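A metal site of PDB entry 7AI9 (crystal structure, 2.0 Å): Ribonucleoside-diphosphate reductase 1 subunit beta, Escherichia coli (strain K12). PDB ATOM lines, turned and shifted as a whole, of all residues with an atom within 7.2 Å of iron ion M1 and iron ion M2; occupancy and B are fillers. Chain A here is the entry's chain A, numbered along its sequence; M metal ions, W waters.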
ATOM      1  N   GLN A  81     -17.772 -31.280  -2.696  1.00  0.00           N
ATOM      2  CA  GLN A  81     -18.349 -29.967  -2.977  1.00  0.00           C
ATOM      3  C   GLN A  81     -19.854 -30.049  -3.092  1.00  0.00           C
ATOM      4  O   GLN A  81     -20.582 -29.234  -2.519  1.00  0.00           O
ATOM      5  CB  GLN A  81     -17.756 -29.400  -4.267  1.00  0.00           C
ATOM      6  CG  GLN A  81     -16.283 -29.046  -4.159  1.00  0.00           C
ATOM      7  CD  GLN A  81     -15.637 -28.645  -5.498  1.00  0.00           C
ATOM      8  OE1 GLN A  81     -15.931 -29.223  -6.535  1.00  0.00           O
ATOM      9  NE2 GLN A  81     -14.711 -27.685  -5.459  1.00  0.00           N
ATOM     10  N   LEU A  84     -21.369 -30.598   0.280  1.00  0.00           N
ATOM     11  CA  LEU A  84     -21.340 -29.404   1.115  1.00  0.00           C
ATOM     12  C   LEU A  84     -22.378 -28.385   0.677  1.00  0.00           C
ATOM     13  O   LEU A  84     -23.006 -27.729   1.522  1.00  0.00           O
ATOM     14  CB  LEU A  84     -19.946 -28.779   1.088  1.00  0.00           C
ATOM     15  CG  LEU A  84     -18.841 -29.536   1.820  1.00  0.00           C
ATOM     16  CD1 LEU A  84     -17.470 -28.847   1.691  1.00  0.00           C
ATOM     17  CD2 LEU A  84     -19.229 -29.716   3.273  1.00  0.00           C
ATOM     18  N   ASP A  85     -22.564 -28.194  -0.621  1.00  0.00           N
ATOM     19  CA  ASP A  85     -23.518 -27.178  -1.018  1.00  0.00           C
ATOM     20  C   ASP A  85     -24.942 -27.704  -1.098  1.00  0.00           C
ATOM     21  O   ASP A  85     -25.882 -26.899  -1.188  1.00  0.00           O
ATOM     22  CB  ASP A  85     -23.071 -26.494  -2.323  1.00  0.00           C
ATOM     23  CG  ASP A  85     -22.208 -25.261  -2.042  1.00  0.00           C
ATOM     24  OD1 ASP A  85     -22.028 -24.937  -0.826  1.00  0.00           O
ATOM     25  OD2 ASP A  85     -21.681 -24.628  -2.968  1.00  0.00           O
ATOM     26  N   GLN A  88     -25.578 -26.428   2.261  1.00  0.00           N
ATOM     27  CA  GLN A  88     -25.564 -24.971   2.288  1.00  0.00           C
ATOM     28  C   GLN A  88     -26.709 -24.366   1.497  1.00  0.00           C
ATOM     29  O   GLN A  88     -27.096 -23.233   1.790  1.00  0.00           O
ATOM     30  CB  GLN A  88     -24.235 -24.448   1.745  1.00  0.00           C
ATOM     31  CG  GLN A  88     -23.099 -24.558   2.729  1.00  0.00           C
ATOM     32  CD  GLN A  88     -23.354 -23.737   3.965  1.00  0.00           C
ATOM     33  OE1 GLN A  88     -23.806 -24.261   4.996  1.00  0.00           O
ATOM     34  NE2 GLN A  88     -23.098 -22.441   3.876  1.00  0.00           N
ATOM     35  N   GLY A  89     -27.223 -25.094   0.515  1.00  0.00           N
ATOM     36  CA  GLY A  89     -28.378 -24.607  -0.233  1.00  0.00           C
ATOM     37  C   GLY A  89     -29.610 -24.419   0.639  1.00  0.00           C
ATOM     38  O   GLY A  89     -30.336 -23.451   0.478  1.00  0.00           O
ATOM     39  N   TRP A 112     -27.848 -15.549   0.113  1.00  0.00           N
ATOM     40  CA  TRP A 112     -26.807 -16.533   0.311  1.00  0.00           C
ATOM     41  C   TRP A 112     -27.249 -17.946  -0.034  1.00  0.00           C
ATOM     42  O   TRP A 112     -26.615 -18.623  -0.857  1.00  0.00           O
ATOM     43  CB  TRP A 112     -26.384 -16.431   1.768  1.00  0.00           C
ATOM     44  CG  TRP A 112     -25.393 -17.425   2.300  1.00  0.00           C
ATOM     45  CD1 TRP A 112     -24.560 -18.244   1.600  1.00  0.00           C
ATOM     46  CD2 TRP A 112     -25.182 -17.694   3.681  1.00  0.00           C
ATOM     47  NE1 TRP A 112     -23.795 -18.994   2.496  1.00  0.00           N
ATOM     48  CE2 TRP A 112     -24.169 -18.676   3.779  1.00  0.00           C
ATOM     49  CE3 TRP A 112     -25.740 -17.172   4.861  1.00  0.00           C
ATOM     50  CZ2 TRP A 112     -23.717 -19.157   5.010  1.00  0.00           C
ATOM     51  CZ3 TRP A 112     -25.296 -17.647   6.081  1.00  0.00           C
ATOM     52  CH2 TRP A 112     -24.282 -18.635   6.138  1.00  0.00           C
ATOM     53  N   SER A 115     -27.853 -18.318  -3.744  1.00  0.00           N
ATOM     54  CA  SER A 115     -26.617 -18.450  -4.507  1.00  0.00           C
ATOM     55  C   SER A 115     -26.040 -19.854  -4.348  1.00  0.00           C
ATOM     56  O   SER A 115     -25.454 -20.400  -5.286  1.00  0.00           O
ATOM     57  CB  SER A 115     -25.649 -17.375  -4.072  1.00  0.00           C
ATOM     58  OG  SER A 115     -25.069 -17.689  -2.800  1.00  0.00           O
ATOM     59  N   GLU A 116     -26.300 -20.506  -3.209  1.00  0.00           N
ATOM     60  CA  GLU A 116     -25.825 -21.877  -3.053  1.00  0.00           C
ATOM     61  C   GLU A 116     -26.568 -22.840  -3.963  1.00  0.00           C
ATOM     62  O   GLU A 116     -25.966 -23.829  -4.402  1.00  0.00           O
ATOM     63  CB  GLU A 116     -25.966 -22.369  -1.616  1.00  0.00           C
ATOM     64  CG  GLU A 116     -25.255 -21.557  -0.545  1.00  0.00           C
ATOM     65  CD  GLU A 116     -23.746 -21.706  -0.587  1.00  0.00           C
ATOM     66  OE1 GLU A 116     -23.220 -22.332  -1.523  1.00  0.00           O
ATOM     67  OE2 GLU A 116     -23.082 -21.247   0.357  1.00  0.00           O
ATOM     68  N   THR A 117     -27.860 -22.591  -4.242  1.00  0.00           N
ATOM     69  CA  THR A 117     -28.546 -23.491  -5.160  1.00  0.00           C
ATOM     70  C   THR A 117     -27.972 -23.356  -6.564  1.00  0.00           C
ATOM     71  O   THR A 117     -27.959 -24.339  -7.311  1.00  0.00           O
ATOM     72  CB  THR A 117     -30.072 -23.270  -5.191  1.00  0.00           C
ATOM     73  OG1 THR A 117     -30.384 -22.011  -5.795  1.00  0.00           O
ATOM     74  CG2 THR A 117     -30.689 -23.358  -3.798  1.00  0.00           C
ATOM     75  N   ILE A 118     -27.502 -22.171  -6.940  1.00  0.00           N
ATOM     76  CA  ILE A 118     -26.811 -22.048  -8.226  1.00  0.00           C
ATOM     77  C   ILE A 118     -25.527 -22.870  -8.196  1.00  0.00           C
ATOM     78  O   ILE A 118     -25.195 -23.566  -9.169  1.00  0.00           O
ATOM     79  CB  ILE A 118     -26.534 -20.563  -8.545  1.00  0.00           C
ATOM     80  CG1 ILE A 118     -27.863 -19.783  -8.622  1.00  0.00           C
ATOM     81  CG2 ILE A 118     -25.737 -20.442  -9.852  1.00  0.00           C
ATOM     82  CD1 ILE A 118     -28.815 -20.285  -9.730  1.00  0.00           C
ATOM     83  N   HIS A 119     -24.812 -22.849  -7.077  1.00  0.00           N
ATOM     84  CA  HIS A 119     -23.642 -23.721  -6.961  1.00  0.00           C
ATOM     85  C   HIS A 119     -24.048 -25.181  -7.130  1.00  0.00           C
ATOM     86  O   HIS A 119     -23.451 -25.917  -7.919  1.00  0.00           O
ATOM     87  CB  HIS A 119     -22.912 -23.497  -5.618  1.00  0.00           C
ATOM     88  CG  HIS A 119     -22.382 -22.115  -5.436  1.00  0.00           C
ATOM     89  ND1 HIS A 119     -21.748 -21.698  -4.284  1.00  0.00           N
ATOM     90  CD2 HIS A 119     -22.399 -21.040  -6.262  1.00  0.00           C
ATOM     91  CE1 HIS A 119     -21.393 -20.427  -4.410  1.00  0.00           C
ATOM     92  NE2 HIS A 119     -21.765 -20.011  -5.600  1.00  0.00           N
ATOM     93  N   SER A 120     -25.111 -25.608  -6.439  1.00  0.00           N
ATOM     94  CA  SER A 120     -25.554 -27.001  -6.557  1.00  0.00           C
ATOM     95  C   SER A 120     -25.962 -27.323  -8.004  1.00  0.00           C
ATOM     96  O   SER A 120     -25.655 -28.413  -8.518  1.00  0.00           O
ATOM     97  CB  SER A 120     -26.715 -27.271  -5.601  1.00  0.00           C
ATOM     98  OG  SER A 120     -26.280 -27.174  -4.251  1.00  0.00           O
ATOM     99  N   TYR A 123     -22.842 -27.942 -10.102  1.00  0.00           N
ATOM    100  CA  TYR A 123     -22.203 -29.251  -9.958  1.00  0.00           C
ATOM    101  C   TYR A 123     -22.936 -30.305 -10.770  1.00  0.00           C
ATOM    102  O   TYR A 123     -22.305 -31.228 -11.301  1.00  0.00           O
ATOM    103  CB  TYR A 123     -22.141 -29.670  -8.480  1.00  0.00           C
ATOM    104  CG  TYR A 123     -21.383 -28.715  -7.595  1.00  0.00           C
ATOM    105  CD1 TYR A 123     -20.110 -28.287  -7.937  1.00  0.00           C
ATOM    106  CD2 TYR A 123     -21.961 -28.214  -6.430  1.00  0.00           C
ATOM    107  CE1 TYR A 123     -19.418 -27.388  -7.137  1.00  0.00           C
ATOM    108  CE2 TYR A 123     -21.286 -27.319  -5.639  1.00  0.00           C
ATOM    109  CZ  TYR A 123     -20.012 -26.905  -5.999  1.00  0.00           C
ATOM    110  OH  TYR A 123     -19.305 -26.029  -5.212  1.00  0.00           O
ATOM    111  N   LEU A 204     -16.744 -24.339   7.294  1.00  0.00           N
ATOM    112  CA  LEU A 204     -17.189 -25.005   6.086  1.00  0.00           C
ATOM    113  C   LEU A 204     -16.831 -24.197   4.852  1.00  0.00           C
ATOM    114  O   LEU A 204     -16.131 -24.678   3.950  1.00  0.00           O
ATOM    115  CB  LEU A 204     -18.715 -25.219   6.125  1.00  0.00           C
ATOM    116  CG  LEU A 204     -19.479 -26.073   5.108  1.00  0.00           C
ATOM    117  CD1 LEU A 204     -20.879 -26.382   5.660  1.00  0.00           C
ATOM    118  CD2 LEU A 204     -19.654 -25.377   3.768  1.00  0.00           C
ATOM    119  N   GLU A 205     -17.310 -22.951   4.796  1.00  0.00           N
ATOM    120  CA  GLU A 205     -17.075 -22.112   3.620  1.00  0.00           C
ATOM    121  C   GLU A 205     -15.646 -21.570   3.553  1.00  0.00           C
ATOM    122  O   GLU A 205     -15.096 -21.451   2.462  1.00  0.00           O
ATOM    123  CB  GLU A 205     -18.079 -20.975   3.614  1.00  0.00           C
ATOM    124  CG  GLU A 205     -19.516 -21.554   3.478  1.00  0.00           C
ATOM    125  CD  GLU A 205     -20.561 -20.495   3.245  1.00  0.00           C
ATOM    126  OE1 GLU A 205     -20.645 -19.546   4.055  1.00  0.00           O
ATOM    127  OE2 GLU A 205     -21.330 -20.622   2.262  1.00  0.00           O
ATOM    128  N   PHE A 209     -14.228 -25.630   1.823  1.00  0.00           N
ATOM    129  CA  PHE A 209     -14.370 -25.380   0.392  1.00  0.00           C
ATOM    130  C   PHE A 209     -13.075 -24.894  -0.239  1.00  0.00           C
ATOM    131  O   PHE A 209     -12.818 -25.189  -1.406  1.00  0.00           O
ATOM    132  CB  PHE A 209     -15.482 -24.371   0.116  1.00  0.00           C
ATOM    133  CG  PHE A 209     -16.761 -25.017  -0.358  1.00  0.00           C
ATOM    134  CD1 PHE A 209     -16.854 -25.556  -1.633  1.00  0.00           C
ATOM    135  CD2 PHE A 209     -17.846 -25.085   0.477  1.00  0.00           C
ATOM    136  CE1 PHE A 209     -17.982 -26.177  -2.051  1.00  0.00           C
ATOM    137  CE2 PHE A 209     -19.031 -25.695   0.048  1.00  0.00           C
ATOM    138  CZ  PHE A 209     -19.095 -26.247  -1.207  1.00  0.00           C
ATOM    139  N   PHE A 213     -11.260 -26.089  -3.577  1.00  0.00           N
ATOM    140  CA  PHE A 213     -10.860 -25.214  -4.666  1.00  0.00           C
ATOM    141  C   PHE A 213      -9.430 -25.504  -5.111  1.00  0.00           C
ATOM    142  O   PHE A 213      -9.143 -25.518  -6.317  1.00  0.00           O
ATOM    143  CB  PHE A 213     -11.007 -23.746  -4.244  1.00  0.00           C
ATOM    144  CG  PHE A 213     -12.423 -23.320  -3.899  1.00  0.00           C
ATOM    145  CD1 PHE A 213     -13.540 -24.024  -4.378  1.00  0.00           C
ATOM    146  CD2 PHE A 213     -12.657 -22.179  -3.139  1.00  0.00           C
ATOM    147  CE1 PHE A 213     -14.848 -23.612  -4.072  1.00  0.00           C
ATOM    148  CE2 PHE A 213     -13.953 -21.757  -2.817  1.00  0.00           C
ATOM    149  CZ  PHE A 213     -15.060 -22.480  -3.303  1.00  0.00           C
ATOM    150  N   ILE A 235     -17.766 -19.904  -8.265  1.00  0.00           N
ATOM    151  CA  ILE A 235     -18.202 -20.369  -6.950  1.00  0.00           C
ATOM    152  C   ILE A 235     -17.329 -19.773  -5.861  1.00  0.00           C
ATOM    153  O   ILE A 235     -17.827 -19.284  -4.835  1.00  0.00           O
ATOM    154  CB  ILE A 235     -18.182 -21.906  -6.929  1.00  0.00           C
ATOM    155  CG1 ILE A 235     -19.332 -22.448  -7.782  1.00  0.00           C
ATOM    156  CG2 ILE A 235     -18.252 -22.442  -5.491  1.00  0.00           C
ATOM    157  CD1 ILE A 235     -19.335 -23.988  -7.868  1.00  0.00           C
ATOM    158  N   ALA A 236     -16.004 -19.773  -6.081  1.00  0.00           N
ATOM    159  CA  ALA A 236     -15.070 -19.242  -5.088  1.00  0.00           C
ATOM    160  C   ALA A 236     -15.297 -17.747  -4.858  1.00  0.00           C
ATOM    161  O   ALA A 236     -15.205 -17.262  -3.723  1.00  0.00           O
ATOM    162  CB  ALA A 236     -13.638 -19.517  -5.545  1.00  0.00           C
ATOM    163  N   ASP A 238     -18.157 -16.252  -5.059  1.00  0.00           N
ATOM    164  CA  ASP A 238     -19.320 -16.207  -4.167  1.00  0.00           C
ATOM    165  C   ASP A 238     -18.921 -16.609  -2.753  1.00  0.00           C
ATOM    166  O   ASP A 238     -19.327 -15.969  -1.764  1.00  0.00           O
ATOM    167  CB  ASP A 238     -20.438 -17.157  -4.657  1.00  0.00           C
ATOM    168  CG  ASP A 238     -21.055 -16.741  -5.981  1.00  0.00           C
ATOM    169  OD1 ASP A 238     -20.975 -15.551  -6.337  1.00  0.00           O
ATOM    170  OD2 ASP A 238     -21.682 -17.633  -6.645  1.00  0.00           O
ATOM    171  N   GLU A 239     -18.123 -17.664  -2.631  1.00  0.00           N
ATOM    172  CA  GLU A 239     -17.754 -18.175  -1.319  1.00  0.00           C
ATOM    173  C   GLU A 239     -17.057 -17.113  -0.467  1.00  0.00           C
ATOM    174  O   GLU A 239     -17.199 -17.111   0.760  1.00  0.00           O
ATOM    175  CB  GLU A 239     -16.847 -19.389  -1.480  1.00  0.00           C
ATOM    176  CG  GLU A 239     -16.717 -20.209  -0.227  1.00  0.00           C
ATOM    177  CD  GLU A 239     -17.998 -20.963   0.012  1.00  0.00           C
ATOM    178  OE1 GLU A 239     -18.915 -20.368   0.600  1.00  0.00           O
ATOM    179  OE2 GLU A 239     -18.115 -22.130  -0.397  1.00  0.00           O
ATOM    180  N   ALA A 240     -16.324 -16.201  -1.106  1.00  0.00           N
ATOM    181  CA  ALA A 240     -15.652 -15.132  -0.385  1.00  0.00           C
ATOM    182  C   ALA A 240     -16.672 -14.194   0.264  1.00  0.00           C
ATOM    183  O   ALA A 240     -16.418 -13.676   1.365  1.00  0.00           O
ATOM    184  CB  ALA A 240     -14.727 -14.360  -1.320  1.00  0.00           C
ATOM    185  N   LEU A 241     -17.804 -13.963  -0.405  1.00  0.00           N
ATOM    186  CA  LEU A 241     -18.908 -13.222   0.187  1.00  0.00           C
ATOM    187  C   LEU A 241     -19.536 -14.003   1.336  1.00  0.00           C
ATOM    188  O   LEU A 241     -19.818 -13.444   2.402  1.00  0.00           O
ATOM    189  CB  LEU A 241     -19.998 -12.923  -0.856  1.00  0.00           C
ATOM    190  CG  LEU A 241     -19.651 -12.117  -2.112  1.00  0.00           C
ATOM    191  CD1 LEU A 241     -20.935 -11.885  -2.935  1.00  0.00           C
ATOM    192  CD2 LEU A 241     -18.924 -10.818  -1.812  1.00  0.00           C
ATOM    193  N   HIS A 242     -19.781 -15.289   1.121  1.00  0.00           N
ATOM    194  CA  HIS A 242     -20.409 -16.102   2.160  1.00  0.00           C
ATOM    195  C   HIS A 242     -19.596 -16.072   3.439  1.00  0.00           C
ATOM    196  O   HIS A 242     -20.119 -15.817   4.533  1.00  0.00           O
ATOM    197  CB  HIS A 242     -20.554 -17.529   1.668  1.00  0.00           C
ATOM    198  CG  HIS A 242     -21.406 -17.642   0.441  1.00  0.00           C
ATOM    199  ND1 HIS A 242     -21.484 -18.797  -0.282  1.00  0.00           N
ATOM    200  CD2 HIS A 242     -22.124 -16.716  -0.229  1.00  0.00           C
ATOM    201  CE1 HIS A 242     -22.296 -18.600  -1.323  1.00  0.00           C
ATOM    202  NE2 HIS A 242     -22.654 -17.332  -1.332  1.00  0.00           N
ATOM    203  N   LEU A 243     -18.312 -16.351   3.341  1.00  0.00           N
ATOM    204  CA  LEU A 243     -17.540 -16.443   4.568  1.00  0.00           C
ATOM    205  C   LEU A 243     -17.378 -15.078   5.215  1.00  0.00           C
ATOM    206  O   LEU A 243     -17.202 -14.978   6.432  1.00  0.00           O
ATOM    207  CB  LEU A 243     -16.209 -17.131   4.265  1.00  0.00           C
ATOM    208  CG  LEU A 243     -15.184 -16.375   3.439  1.00  0.00           C
ATOM    209  CD1 LEU A 243     -14.323 -15.538   4.396  1.00  0.00           C
ATOM    210  CD2 LEU A 243     -14.316 -17.352   2.700  1.00  0.00           C
HETATM  211 FE    FE M   1     -20.974 -20.809   0.295  1.00  0.00          FE
HETATM  212 FE    FE M   2     -21.381 -22.786  -2.451  1.00  0.00          FE
HETATM  213  O   HOH W   1     -20.783 -22.736   0.286  1.00  0.00           O
HETATM  214  O   HOH W   2     -20.675 -21.240  -1.671  1.00  0.00           O
HETATM  215  O   HOH W   3     -19.247 -23.418  -2.721  1.00  0.00           O
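O of Glu 116 lies within hydrogen-bond range of OG of Ser 120 (3.4 Å).
The side-chain carboxylate (OE2) of Glu 205 lies close to the side-chain amide nitrogen (NE2) of Gln 88 (3.0 Å).
The side-chain hydroxyl (OG) of Ser 120 sits at hydrogen-bond distance from the backbone carbonyl oxygen (O) of Asp 85, at 3.1 Å.
OE2 of Glu 116 lies close to NE1 of Trp 112 (3.2 Å).
OE2 of Glu 205 sits close to NE1 of Trp 112 (3.0 Å).
A ring nitrogen (NE2) of His 119 sits at hydrogen-bond distance from the side-chain carboxylate of Asp 238, 2.6 Å away.
OG of Ser 115 sits at hydrogen-bond distance from NE2 of His 242 (2.8 Å).
Of the 25 residues printed, 4 come within 4 Å of iron ion M1.
Four residues have an atom within 4 Å of iron ion M2: Asp 85, Glu 116, His 119 and Glu 239.
Iron ion M1 is bound by water W1 (1.9 Å), the side-chain carboxylate (OE2) of Glu 205 (2.0 Å), water W2 (2.0 Å), the side-chain carboxylate (OE1) of Glu 239 (2.1 Å), the side-chain carboxylate (OE2) of Glu 116 (2.2 Å) and a ring nitrogen (ND1) of His 242 (2.2 Å).
Iron ion M1 has six donor atoms within binding distance.
Iron ion M2 is bound by water W2 (1.9 Å), OD2 of Asp 85 (1.9 Å), OE1 of Glu 116 (2.1 Å), ND1 of His 119 (2.2 Å) and water W3 (2.2 Å).
Iron ion M2 has five donor atoms within binding distance.
Slightly farther from iron ion M2 lies OD1 of Asp 85 (2.8 Å).
Slightly farther from iron ion M2 lies water W1 (2.8 Å).
Water W1 bridges OD1 of Asp 85 (2.8 Å) and OE2 of Glu 239 (2.8 Å).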
